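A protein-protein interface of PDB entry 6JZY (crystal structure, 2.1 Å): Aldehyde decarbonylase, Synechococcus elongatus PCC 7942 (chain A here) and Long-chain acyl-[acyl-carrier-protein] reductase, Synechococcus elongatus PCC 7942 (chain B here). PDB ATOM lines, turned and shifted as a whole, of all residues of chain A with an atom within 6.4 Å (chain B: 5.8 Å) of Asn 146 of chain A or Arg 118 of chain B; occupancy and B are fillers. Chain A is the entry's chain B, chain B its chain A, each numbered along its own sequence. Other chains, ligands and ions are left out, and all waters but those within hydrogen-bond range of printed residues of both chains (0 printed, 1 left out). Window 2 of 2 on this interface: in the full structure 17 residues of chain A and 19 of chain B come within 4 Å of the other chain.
Printed residues of chain A that touch a printed residue of chain B: Asn 146, Tyr 168, Ser 220, Glu 223, Asp 224 and Ile 227.
Printed residues of chain B that touch a printed residue of chain A: Arg 79, Asn 83, Arg 118 and Asp 119.
Among the printed residues, 8 pairs touch across the chains.
The side-chain hydroxyl (OG) of Ser 220 of chain A lies within hydrogen-bond range of the guanidinium group (NH1) of Arg 79 of chain B (3.3 Å).
NE of Arg 79 of chain B lies within salt-bridge range of OE2 of Glu 223 of chain A (2.7 Å).
ND2 of Asn 83 of chain B sits at hydrogen-bond distance from OE2 of Glu 223 of chain A, at 2.8 Å.
NE of Arg 118 of chain B is in salt-bridge range of OD2 of Asp 224 of chain A, 2.7 Å away.
OH of Tyr 168 of chain A sits close to OD1 of Asp 119 of chain B (3.5 Å).
Of chain B, only Arg 118 comes within 4 Å of Asn 146 of chain A.
Printed residues of chain A within 4 Å of Asn 83 of chain B: Glu 223 (2.8 Å) and Ile 227 (3.8 Å).
Printed residues of chain A within 4 Å of Arg 79 of chain B: Ser 220 (3.3 Å) and Glu 223 (2.7 Å).
Printed residues of chain B within 4 Å of Ile 227 of chain A: Asn 83 (3.8 Å) and Arg 118 (3.4 Å).
Ile 149 of chain A touches none of the printed residues of chain B.
Val 117 of chain B touches none of the printed residues of chain A.
The nearest residue of chain A that does not touch Arg 118 of chain B is Glu 223 of chain A (4.2 Å).
The backbone carbonyl oxygen (O) of Arg 79 of chain B lies close to the side-chain amide nitrogen (ND2) of Asn 83 of chain B, 3.1 Å away.
OD1 of Asn 83 of chain B is in hydrogen-bond range of NH2 of Arg 118 of chain B (3.0 Å).
ND2 of Asn 146 of chain A sits close to O of Ile 142 of chain A, 3.4 Å away.
Arg 118 of chain B touches Asn 146 of chain A.
CG of Asn 83 of chain B touches CD1 of Ile 227 of chain A, 3.8 Å away.
Ile 227 of chain A touches Arg 118 of chain B.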
ATOM      1  N   ALA A 141     -29.272  11.051  -9.726  1.00  0.00           N
ATOM      2  CA  ALA A 141     -29.193  11.530  -8.348  1.00  0.00           C
ATOM      3  C   ALA A 141     -27.756  11.836  -7.955  1.00  0.00           C
ATOM      4  O   ALA A 141     -27.483  12.863  -7.330  1.00  0.00           O
ATOM      5  CB  ALA A 141     -29.801  10.495  -7.398  1.00  0.00           C
ATOM      6  N   ILE A 142     -26.827  10.942  -8.304  1.00  0.00           N
ATOM      7  CA  ILE A 142     -25.404  11.163  -8.039  1.00  0.00           C
ATOM      8  C   ILE A 142     -24.947  12.485  -8.641  1.00  0.00           C
ATOM      9  O   ILE A 142     -24.349  13.326  -7.962  1.00  0.00           O
ATOM     10  CB  ILE A 142     -24.578   9.981  -8.576  1.00  0.00           C
ATOM     11  CG1 ILE A 142     -24.831   8.751  -7.714  1.00  0.00           C
ATOM     12  CG2 ILE A 142     -23.098  10.335  -8.626  1.00  0.00           C
ATOM     13  CD1 ILE A 142     -24.397   7.449  -8.351  1.00  0.00           C
ATOM     14  N   ALA A 143     -25.256  12.702  -9.921  1.00  0.00           N
ATOM     15  CA  ALA A 143     -24.909  13.964 -10.568  1.00  0.00           C
ATOM     16  C   ALA A 143     -25.551  15.147  -9.856  1.00  0.00           C
ATOM     17  O   ALA A 143     -24.894  16.160  -9.589  1.00  0.00           O
ATOM     18  CB  ALA A 143     -25.342  13.944 -12.034  1.00  0.00           C
ATOM     19  N   ALA A 144     -26.849  15.038  -9.561  1.00  0.00           N
ATOM     20  CA  ALA A 144     -27.588  16.171  -9.013  1.00  0.00           C
ATOM     21  C   ALA A 144     -27.058  16.559  -7.641  1.00  0.00           C
ATOM     22  O   ALA A 144     -26.887  17.743  -7.337  1.00  0.00           O
ATOM     23  CB  ALA A 144     -29.072  15.823  -8.942  1.00  0.00           C
ATOM     24  N   TYR A 145     -26.771  15.564  -6.806  1.00  0.00           N
ATOM     25  CA  TYR A 145     -26.353  15.844  -5.439  1.00  0.00           C
ATOM     26  C   TYR A 145     -24.895  16.293  -5.394  1.00  0.00           C
ATOM     27  O   TYR A 145     -24.557  17.256  -4.694  1.00  0.00           O
ATOM     28  CB  TYR A 145     -26.583  14.605  -4.575  1.00  0.00           C
ATOM     29  CG  TYR A 145     -28.021  14.138  -4.508  1.00  0.00           C
ATOM     30  CD1 TYR A 145     -29.075  15.013  -4.748  1.00  0.00           C
ATOM     31  CD2 TYR A 145     -28.328  12.813  -4.215  1.00  0.00           C
ATOM     32  CE1 TYR A 145     -30.399  14.579  -4.696  1.00  0.00           C
ATOM     33  CE2 TYR A 145     -29.648  12.371  -4.160  1.00  0.00           C
ATOM     34  CZ  TYR A 145     -30.674  13.261  -4.407  1.00  0.00           C
ATOM     35  OH  TYR A 145     -31.976  12.837  -4.361  1.00  0.00           O
ATOM     36  N   ASN A 146     -24.018  15.612  -6.145  1.00  0.00           N
ATOM     37  CA  ASN A 146     -22.620  16.039  -6.248  1.00  0.00           C
ATOM     38  C   ASN A 146     -22.523  17.524  -6.572  1.00  0.00           C
ATOM     39  O   ASN A 146     -21.786  18.270  -5.923  1.00  0.00           O
ATOM     40  CB  ASN A 146     -21.894  15.235  -7.328  1.00  0.00           C
ATOM     41  CG  ASN A 146     -21.389  13.909  -6.830  1.00  0.00           C
ATOM     42  OD1 ASN A 146     -21.391  13.638  -5.627  1.00  0.00           O
ATOM     43  ND2 ASN A 146     -20.941  13.066  -7.759  1.00  0.00           N
ATOM     44  N   ILE A 147     -23.282  17.967  -7.572  1.00  0.00           N
ATOM     45  CA  ILE A 147     -23.265  19.367  -7.975  1.00  0.00           C
ATOM     46  C   ILE A 147     -23.921  20.260  -6.916  1.00  0.00           C
ATOM     47  O   ILE A 147     -23.608  21.455  -6.824  1.00  0.00           O
ATOM     48  CB  ILE A 147     -23.942  19.485  -9.355  1.00  0.00           C
ATOM     49  CG1 ILE A 147     -23.196  18.633 -10.390  1.00  0.00           C
ATOM     50  CG2 ILE A 147     -24.011  20.919  -9.813  1.00  0.00           C
ATOM     51  CD1 ILE A 147     -21.694  18.809 -10.357  1.00  0.00           C
ATOM     52  N   TYR A 148     -24.825  19.702  -6.097  1.00  0.00           N
ATOM     53  CA  TYR A 148     -25.554  20.484  -5.094  1.00  0.00           C
ATOM     54  C   TYR A 148     -24.687  20.822  -3.888  1.00  0.00           C
ATOM     55  O   TYR A 148     -24.683  21.966  -3.423  1.00  0.00           O
ATOM     56  CB  TYR A 148     -26.812  19.729  -4.627  1.00  0.00           C
ATOM     57  CG  TYR A 148     -27.710  20.548  -3.707  1.00  0.00           C
ATOM     58  CD1 TYR A 148     -27.964  21.884  -3.971  1.00  0.00           C
ATOM     59  CD2 TYR A 148     -28.289  19.988  -2.574  1.00  0.00           C
ATOM     60  CE1 TYR A 148     -28.764  22.646  -3.140  1.00  0.00           C
ATOM     61  CE2 TYR A 148     -29.098  20.747  -1.734  1.00  0.00           C
ATOM     62  CZ  TYR A 148     -29.328  22.076  -2.028  1.00  0.00           C
ATOM     63  OH  TYR A 148     -30.116  22.862  -1.219  1.00  0.00           O
ATOM     64  N   ILE A 149     -23.963  19.832  -3.375  1.00  0.00           N
ATOM     65  CA  ILE A 149     -23.193  19.897  -2.133  1.00  0.00           C
ATOM     66  C   ILE A 149     -22.292  21.132  -2.040  1.00  0.00           C
ATOM     67  O   ILE A 149     -22.283  21.783  -0.986  1.00  0.00           O
ATOM     68  CB  ILE A 149     -22.392  18.595  -1.954  1.00  0.00           C
ATOM     69  CG1 ILE A 149     -23.320  17.488  -1.449  1.00  0.00           C
ATOM     70  CG2 ILE A 149     -21.201  18.800  -1.030  1.00  0.00           C
ATOM     71  CD1 ILE A 149     -22.715  16.086  -1.476  1.00  0.00           C
ATOM     72  N   PRO A 150     -21.537  21.522  -3.079  1.00  0.00           N
ATOM     73  CA  PRO A 150     -20.677  22.711  -2.940  1.00  0.00           C
ATOM     74  C   PRO A 150     -21.429  24.034  -2.907  1.00  0.00           C
ATOM     75  O   PRO A 150     -20.792  25.067  -2.665  1.00  0.00           O
ATOM     76  CB  PRO A 150     -19.762  22.639  -4.177  1.00  0.00           C
ATOM     77  CG  PRO A 150     -19.896  21.256  -4.697  1.00  0.00           C
ATOM     78  CD  PRO A 150     -21.304  20.863  -4.376  1.00  0.00           C
ATOM     79  N   THR A 160     -27.485  16.194   2.033  1.00  0.00           N
ATOM     80  CA  THR A 160     -27.070  15.697   0.727  1.00  0.00           C
ATOM     81  C   THR A 160     -25.785  14.877   0.824  1.00  0.00           C
ATOM     82  O   THR A 160     -25.639  13.853   0.147  1.00  0.00           O
ATOM     83  CB  THR A 160     -26.896  16.877  -0.235  1.00  0.00           C
ATOM     84  OG1 THR A 160     -28.064  17.709  -0.194  1.00  0.00           O
ATOM     85  CG2 THR A 160     -26.688  16.392  -1.647  1.00  0.00           C
ATOM     86  N   VAL A 164     -25.631  10.756  -0.797  1.00  0.00           N
ATOM     87  CA  VAL A 164     -24.871  10.464  -2.014  1.00  0.00           C
ATOM     88  C   VAL A 164     -24.148   9.133  -1.903  1.00  0.00           C
ATOM     89  O   VAL A 164     -23.975   8.428  -2.909  1.00  0.00           O
ATOM     90  CB  VAL A 164     -23.870  11.594  -2.345  1.00  0.00           C
ATOM     91  CG1 VAL A 164     -24.576  12.903  -2.496  1.00  0.00           C
ATOM     92  CG2 VAL A 164     -22.771  11.693  -1.293  1.00  0.00           C
ATOM     93  N   TYR A 168     -24.502   5.493  -4.510  1.00  0.00           N
ATOM     94  CA  TYR A 168     -23.432   4.726  -5.136  1.00  0.00           C
ATOM     95  C   TYR A 168     -23.595   3.222  -4.912  1.00  0.00           C
ATOM     96  O   TYR A 168     -23.334   2.440  -5.835  1.00  0.00           O
ATOM     97  CB  TYR A 168     -22.073   5.216  -4.633  1.00  0.00           C
ATOM     98  CG  TYR A 168     -21.524   6.395  -5.413  1.00  0.00           C
ATOM     99  CD1 TYR A 168     -21.050   6.236  -6.714  1.00  0.00           C
ATOM    100  CD2 TYR A 168     -21.475   7.665  -4.849  1.00  0.00           C
ATOM    101  CE1 TYR A 168     -20.546   7.318  -7.433  1.00  0.00           C
ATOM    102  CE2 TYR A 168     -20.970   8.744  -5.553  1.00  0.00           C
ATOM    103  CZ  TYR A 168     -20.509   8.569  -6.841  1.00  0.00           C
ATOM    104  OH  TYR A 168     -20.016   9.653  -7.532  1.00  0.00           O
ATOM    105  N   SER A 220     -22.064  20.987 -15.877  1.00  0.00           N
ATOM    106  CA  SER A 220     -21.538  20.085 -14.853  1.00  0.00           C
ATOM    107  C   SER A 220     -22.477  18.921 -14.577  1.00  0.00           C
ATOM    108  O   SER A 220     -22.016  17.820 -14.248  1.00  0.00           O
ATOM    109  CB  SER A 220     -21.283  20.839 -13.542  1.00  0.00           C
ATOM    110  OG  SER A 220     -19.949  21.310 -13.457  1.00  0.00           O
ATOM    111  N   GLU A 223     -22.051  16.262 -17.213  1.00  0.00           N
ATOM    112  CA  GLU A 223     -20.746  15.624 -17.078  1.00  0.00           C
ATOM    113  C   GLU A 223     -20.738  14.606 -15.949  1.00  0.00           C
ATOM    114  O   GLU A 223     -20.305  13.462 -16.133  1.00  0.00           O
ATOM    115  CB  GLU A 223     -19.693  16.703 -16.838  1.00  0.00           C
ATOM    116  CG  GLU A 223     -18.267  16.236 -16.764  1.00  0.00           C
ATOM    117  CD  GLU A 223     -17.352  17.433 -16.621  1.00  0.00           C
ATOM    118  OE1 GLU A 223     -17.044  18.056 -17.657  1.00  0.00           O
ATOM    119  OE2 GLU A 223     -16.994  17.768 -15.470  1.00  0.00           O
ATOM    120  N   ASP A 224     -21.196  15.011 -14.761  1.00  0.00           N
ATOM    121  CA  ASP A 224     -21.277  14.080 -13.641  1.00  0.00           C
ATOM    122  C   ASP A 224     -22.218  12.921 -13.957  1.00  0.00           C
ATOM    123  O   ASP A 224     -21.925  11.765 -13.628  1.00  0.00           O
ATOM    124  CB  ASP A 224     -21.719  14.831 -12.385  1.00  0.00           C
ATOM    125  CG  ASP A 224     -20.546  15.475 -11.656  1.00  0.00           C
ATOM    126  OD1 ASP A 224     -20.032  16.508 -12.135  1.00  0.00           O
ATOM    127  OD2 ASP A 224     -20.091  14.916 -10.638  1.00  0.00           O
ATOM    128  N   ILE A 227     -20.319  10.667 -16.307  1.00  0.00           N
ATOM    129  CA  ILE A 227     -19.271   9.953 -15.573  1.00  0.00           C
ATOM    130  C   ILE A 227     -19.875   8.801 -14.767  1.00  0.00           C
ATOM    131  O   ILE A 227     -19.417   7.653 -14.838  1.00  0.00           O
ATOM    132  CB  ILE A 227     -18.496  10.922 -14.659  1.00  0.00           C
ATOM    133  CG1 ILE A 227     -17.494  11.757 -15.460  1.00  0.00           C
ATOM    134  CG2 ILE A 227     -17.725  10.135 -13.605  1.00  0.00           C
ATOM    135  CD1 ILE A 227     -16.772  12.774 -14.623  1.00  0.00           C
ATOM    136  N   ARG B  79     -12.077  20.991 -14.696  1.00  0.00           N
ATOM    137  CA  ARG B  79     -12.761  19.709 -14.513  1.00  0.00           C
ATOM    138  C   ARG B  79     -12.197  18.636 -15.446  1.00  0.00           C
ATOM    139  O   ARG B  79     -12.094  17.460 -15.067  1.00  0.00           O
ATOM    140  CB  ARG B  79     -14.270  19.885 -14.731  1.00  0.00           C
ATOM    141  CG  ARG B  79     -14.981  20.879 -13.768  1.00  0.00           C
ATOM    142  CD  ARG B  79     -16.528  20.693 -13.813  1.00  0.00           C
ATOM    143  NE  ARG B  79     -16.965  20.411 -15.184  1.00  0.00           N
ATOM    144  CZ  ARG B  79     -17.506  21.289 -16.028  1.00  0.00           C
ATOM    145  NH1 ARG B  79     -17.743  22.530 -15.649  1.00  0.00           N
ATOM    146  NH2 ARG B  79     -17.813  20.922 -17.262  1.00  0.00           N
ATOM    147  N   LEU B  82      -9.038  17.282 -13.591  1.00  0.00           N
ATOM    148  CA  LEU B  82      -9.374  16.526 -12.380  1.00  0.00           C
ATOM    149  C   LEU B  82     -10.129  15.238 -12.714  1.00  0.00           C
ATOM    150  O   LEU B  82      -9.842  14.168 -12.158  1.00  0.00           O
ATOM    151  CB  LEU B  82     -10.195  17.402 -11.428  1.00  0.00           C
ATOM    152  CG  LEU B  82      -9.510  18.688 -10.942  1.00  0.00           C
ATOM    153  CD1 LEU B  82     -10.510  19.636 -10.297  1.00  0.00           C
ATOM    154  CD2 LEU B  82      -8.435  18.338  -9.958  1.00  0.00           C
ATOM    155  N   ASN B  83     -11.085  15.313 -13.637  1.00  0.00           N
ATOM    156  CA  ASN B  83     -11.842  14.112 -13.996  1.00  0.00           C
ATOM    157  C   ASN B  83     -10.927  13.063 -14.607  1.00  0.00           C
ATOM    158  O   ASN B  83     -11.040  11.871 -14.298  1.00  0.00           O
ATOM    159  CB  ASN B  83     -12.963  14.445 -14.975  1.00  0.00           C
ATOM    160  CG  ASN B  83     -14.012  15.376 -14.390  1.00  0.00           C
ATOM    161  OD1 ASN B  83     -14.129  15.529 -13.167  1.00  0.00           O
ATOM    162  ND2 ASN B  83     -14.784  16.011 -15.271  1.00  0.00           N
ATOM    163  N   SER B  86      -8.721  11.617 -11.758  1.00  0.00           N
ATOM    164  CA  SER B  86      -9.568  10.703 -10.993  1.00  0.00           C
ATOM    165  C   SER B  86      -9.788   9.404 -11.752  1.00  0.00           C
ATOM    166  O   SER B  86      -9.720   8.311 -11.172  1.00  0.00           O
ATOM    167  CB  SER B  86     -10.906  11.368 -10.687  1.00  0.00           C
ATOM    168  OG  SER B  86     -11.780  10.471 -10.041  1.00  0.00           O
ATOM    169  N   GLN B 116      -9.770  16.580  -3.964  1.00  0.00           N
ATOM    170  CA  GLN B 116     -10.975  15.854  -3.571  1.00  0.00           C
ATOM    171  C   GLN B 116     -11.938  15.874  -4.749  1.00  0.00           C
ATOM    172  O   GLN B 116     -12.612  16.873  -4.999  1.00  0.00           O
ATOM    173  CB  GLN B 116     -11.600  16.472  -2.328  1.00  0.00           C
ATOM    174  CG  GLN B 116     -12.080  15.438  -1.329  1.00  0.00           C
ATOM    175  CD  GLN B 116     -10.993  14.453  -0.946  1.00  0.00           C
ATOM    176  OE1 GLN B 116      -9.948  14.836  -0.404  1.00  0.00           O
ATOM    177  NE2 GLN B 116     -11.228  13.175  -1.235  1.00  0.00           N
ATOM    178  N   VAL B 117     -11.990  14.775  -5.482  1.00  0.00           N
ATOM    179  CA  VAL B 117     -12.736  14.689  -6.733  1.00  0.00           C
ATOM    180  C   VAL B 117     -13.773  13.589  -6.541  1.00  0.00           C
ATOM    181  O   VAL B 117     -13.475  12.402  -6.696  1.00  0.00           O
ATOM    182  CB  VAL B 117     -11.826  14.409  -7.933  1.00  0.00           C
ATOM    183  CG1 VAL B 117     -12.655  14.172  -9.184  1.00  0.00           C
ATOM    184  CG2 VAL B 117     -10.873  15.578  -8.157  1.00  0.00           C
ATOM    185  N   ARG B 118     -15.002  13.983  -6.191  1.00  0.00           N
ATOM    186  CA  ARG B 118     -16.113  13.051  -5.928  1.00  0.00           C
ATOM    187  C   ARG B 118     -15.681  12.059  -4.856  1.00  0.00           C
ATOM    188  O   ARG B 118     -15.359  12.489  -3.737  1.00  0.00           O
ATOM    189  CB  ARG B 118     -16.564  12.427  -7.246  1.00  0.00           C
ATOM    190  CG  ARG B 118     -16.991  13.431  -8.261  1.00  0.00           C
ATOM    191  CD  ARG B 118     -17.496  12.769  -9.526  1.00  0.00           C
ATOM    192  NE  ARG B 118     -17.677  13.799 -10.542  1.00  0.00           N
ATOM    193  CZ  ARG B 118     -16.712  14.199 -11.360  1.00  0.00           C
ATOM    194  NH1 ARG B 118     -15.515  13.631 -11.300  1.00  0.00           N
ATOM    195  NH2 ARG B 118     -16.942  15.161 -12.235  1.00  0.00           N
ATOM    196  N   ASP B 119     -15.651  10.757  -5.132  1.00  0.00           N
ATOM    197  CA  ASP B 119     -15.200   9.808  -4.121  1.00  0.00           C
ATOM    198  C   ASP B 119     -13.722   9.992  -3.821  1.00  0.00           C
ATOM    199  O   ASP B 119     -13.298   9.893  -2.660  1.00  0.00           O
ATOM    200  CB  ASP B 119     -15.460   8.377  -4.589  1.00  0.00           C
ATOM    201  CG  ASP B 119     -16.857   8.188  -5.131  1.00  0.00           C
ATOM    202  OD1 ASP B 119     -17.651   9.150  -5.061  1.00  0.00           O
ATOM    203  OD2 ASP B 119     -17.160   7.080  -5.628  1.00  0.00           O
ATOM    204  N   THR B 120     -12.936  10.305  -4.849  1.00  0.00           N
ATOM    205  CA  THR B 120     -11.500  10.088  -4.838  1.00  0.00           C
ATOM    206  C   THR B 120     -10.746  11.270  -4.237  1.00  0.00           C
ATOM    207  O   THR B 120     -11.136  12.435  -4.377  1.00  0.00           O
ATOM    208  CB  THR B 120     -11.003   9.822  -6.267  1.00  0.00           C
ATOM    209  OG1 THR B 120     -11.163  10.995  -7.077  1.00  0.00           O
ATOM    210  CG2 THR B 120     -11.807   8.693  -6.900  1.00  0.00           C
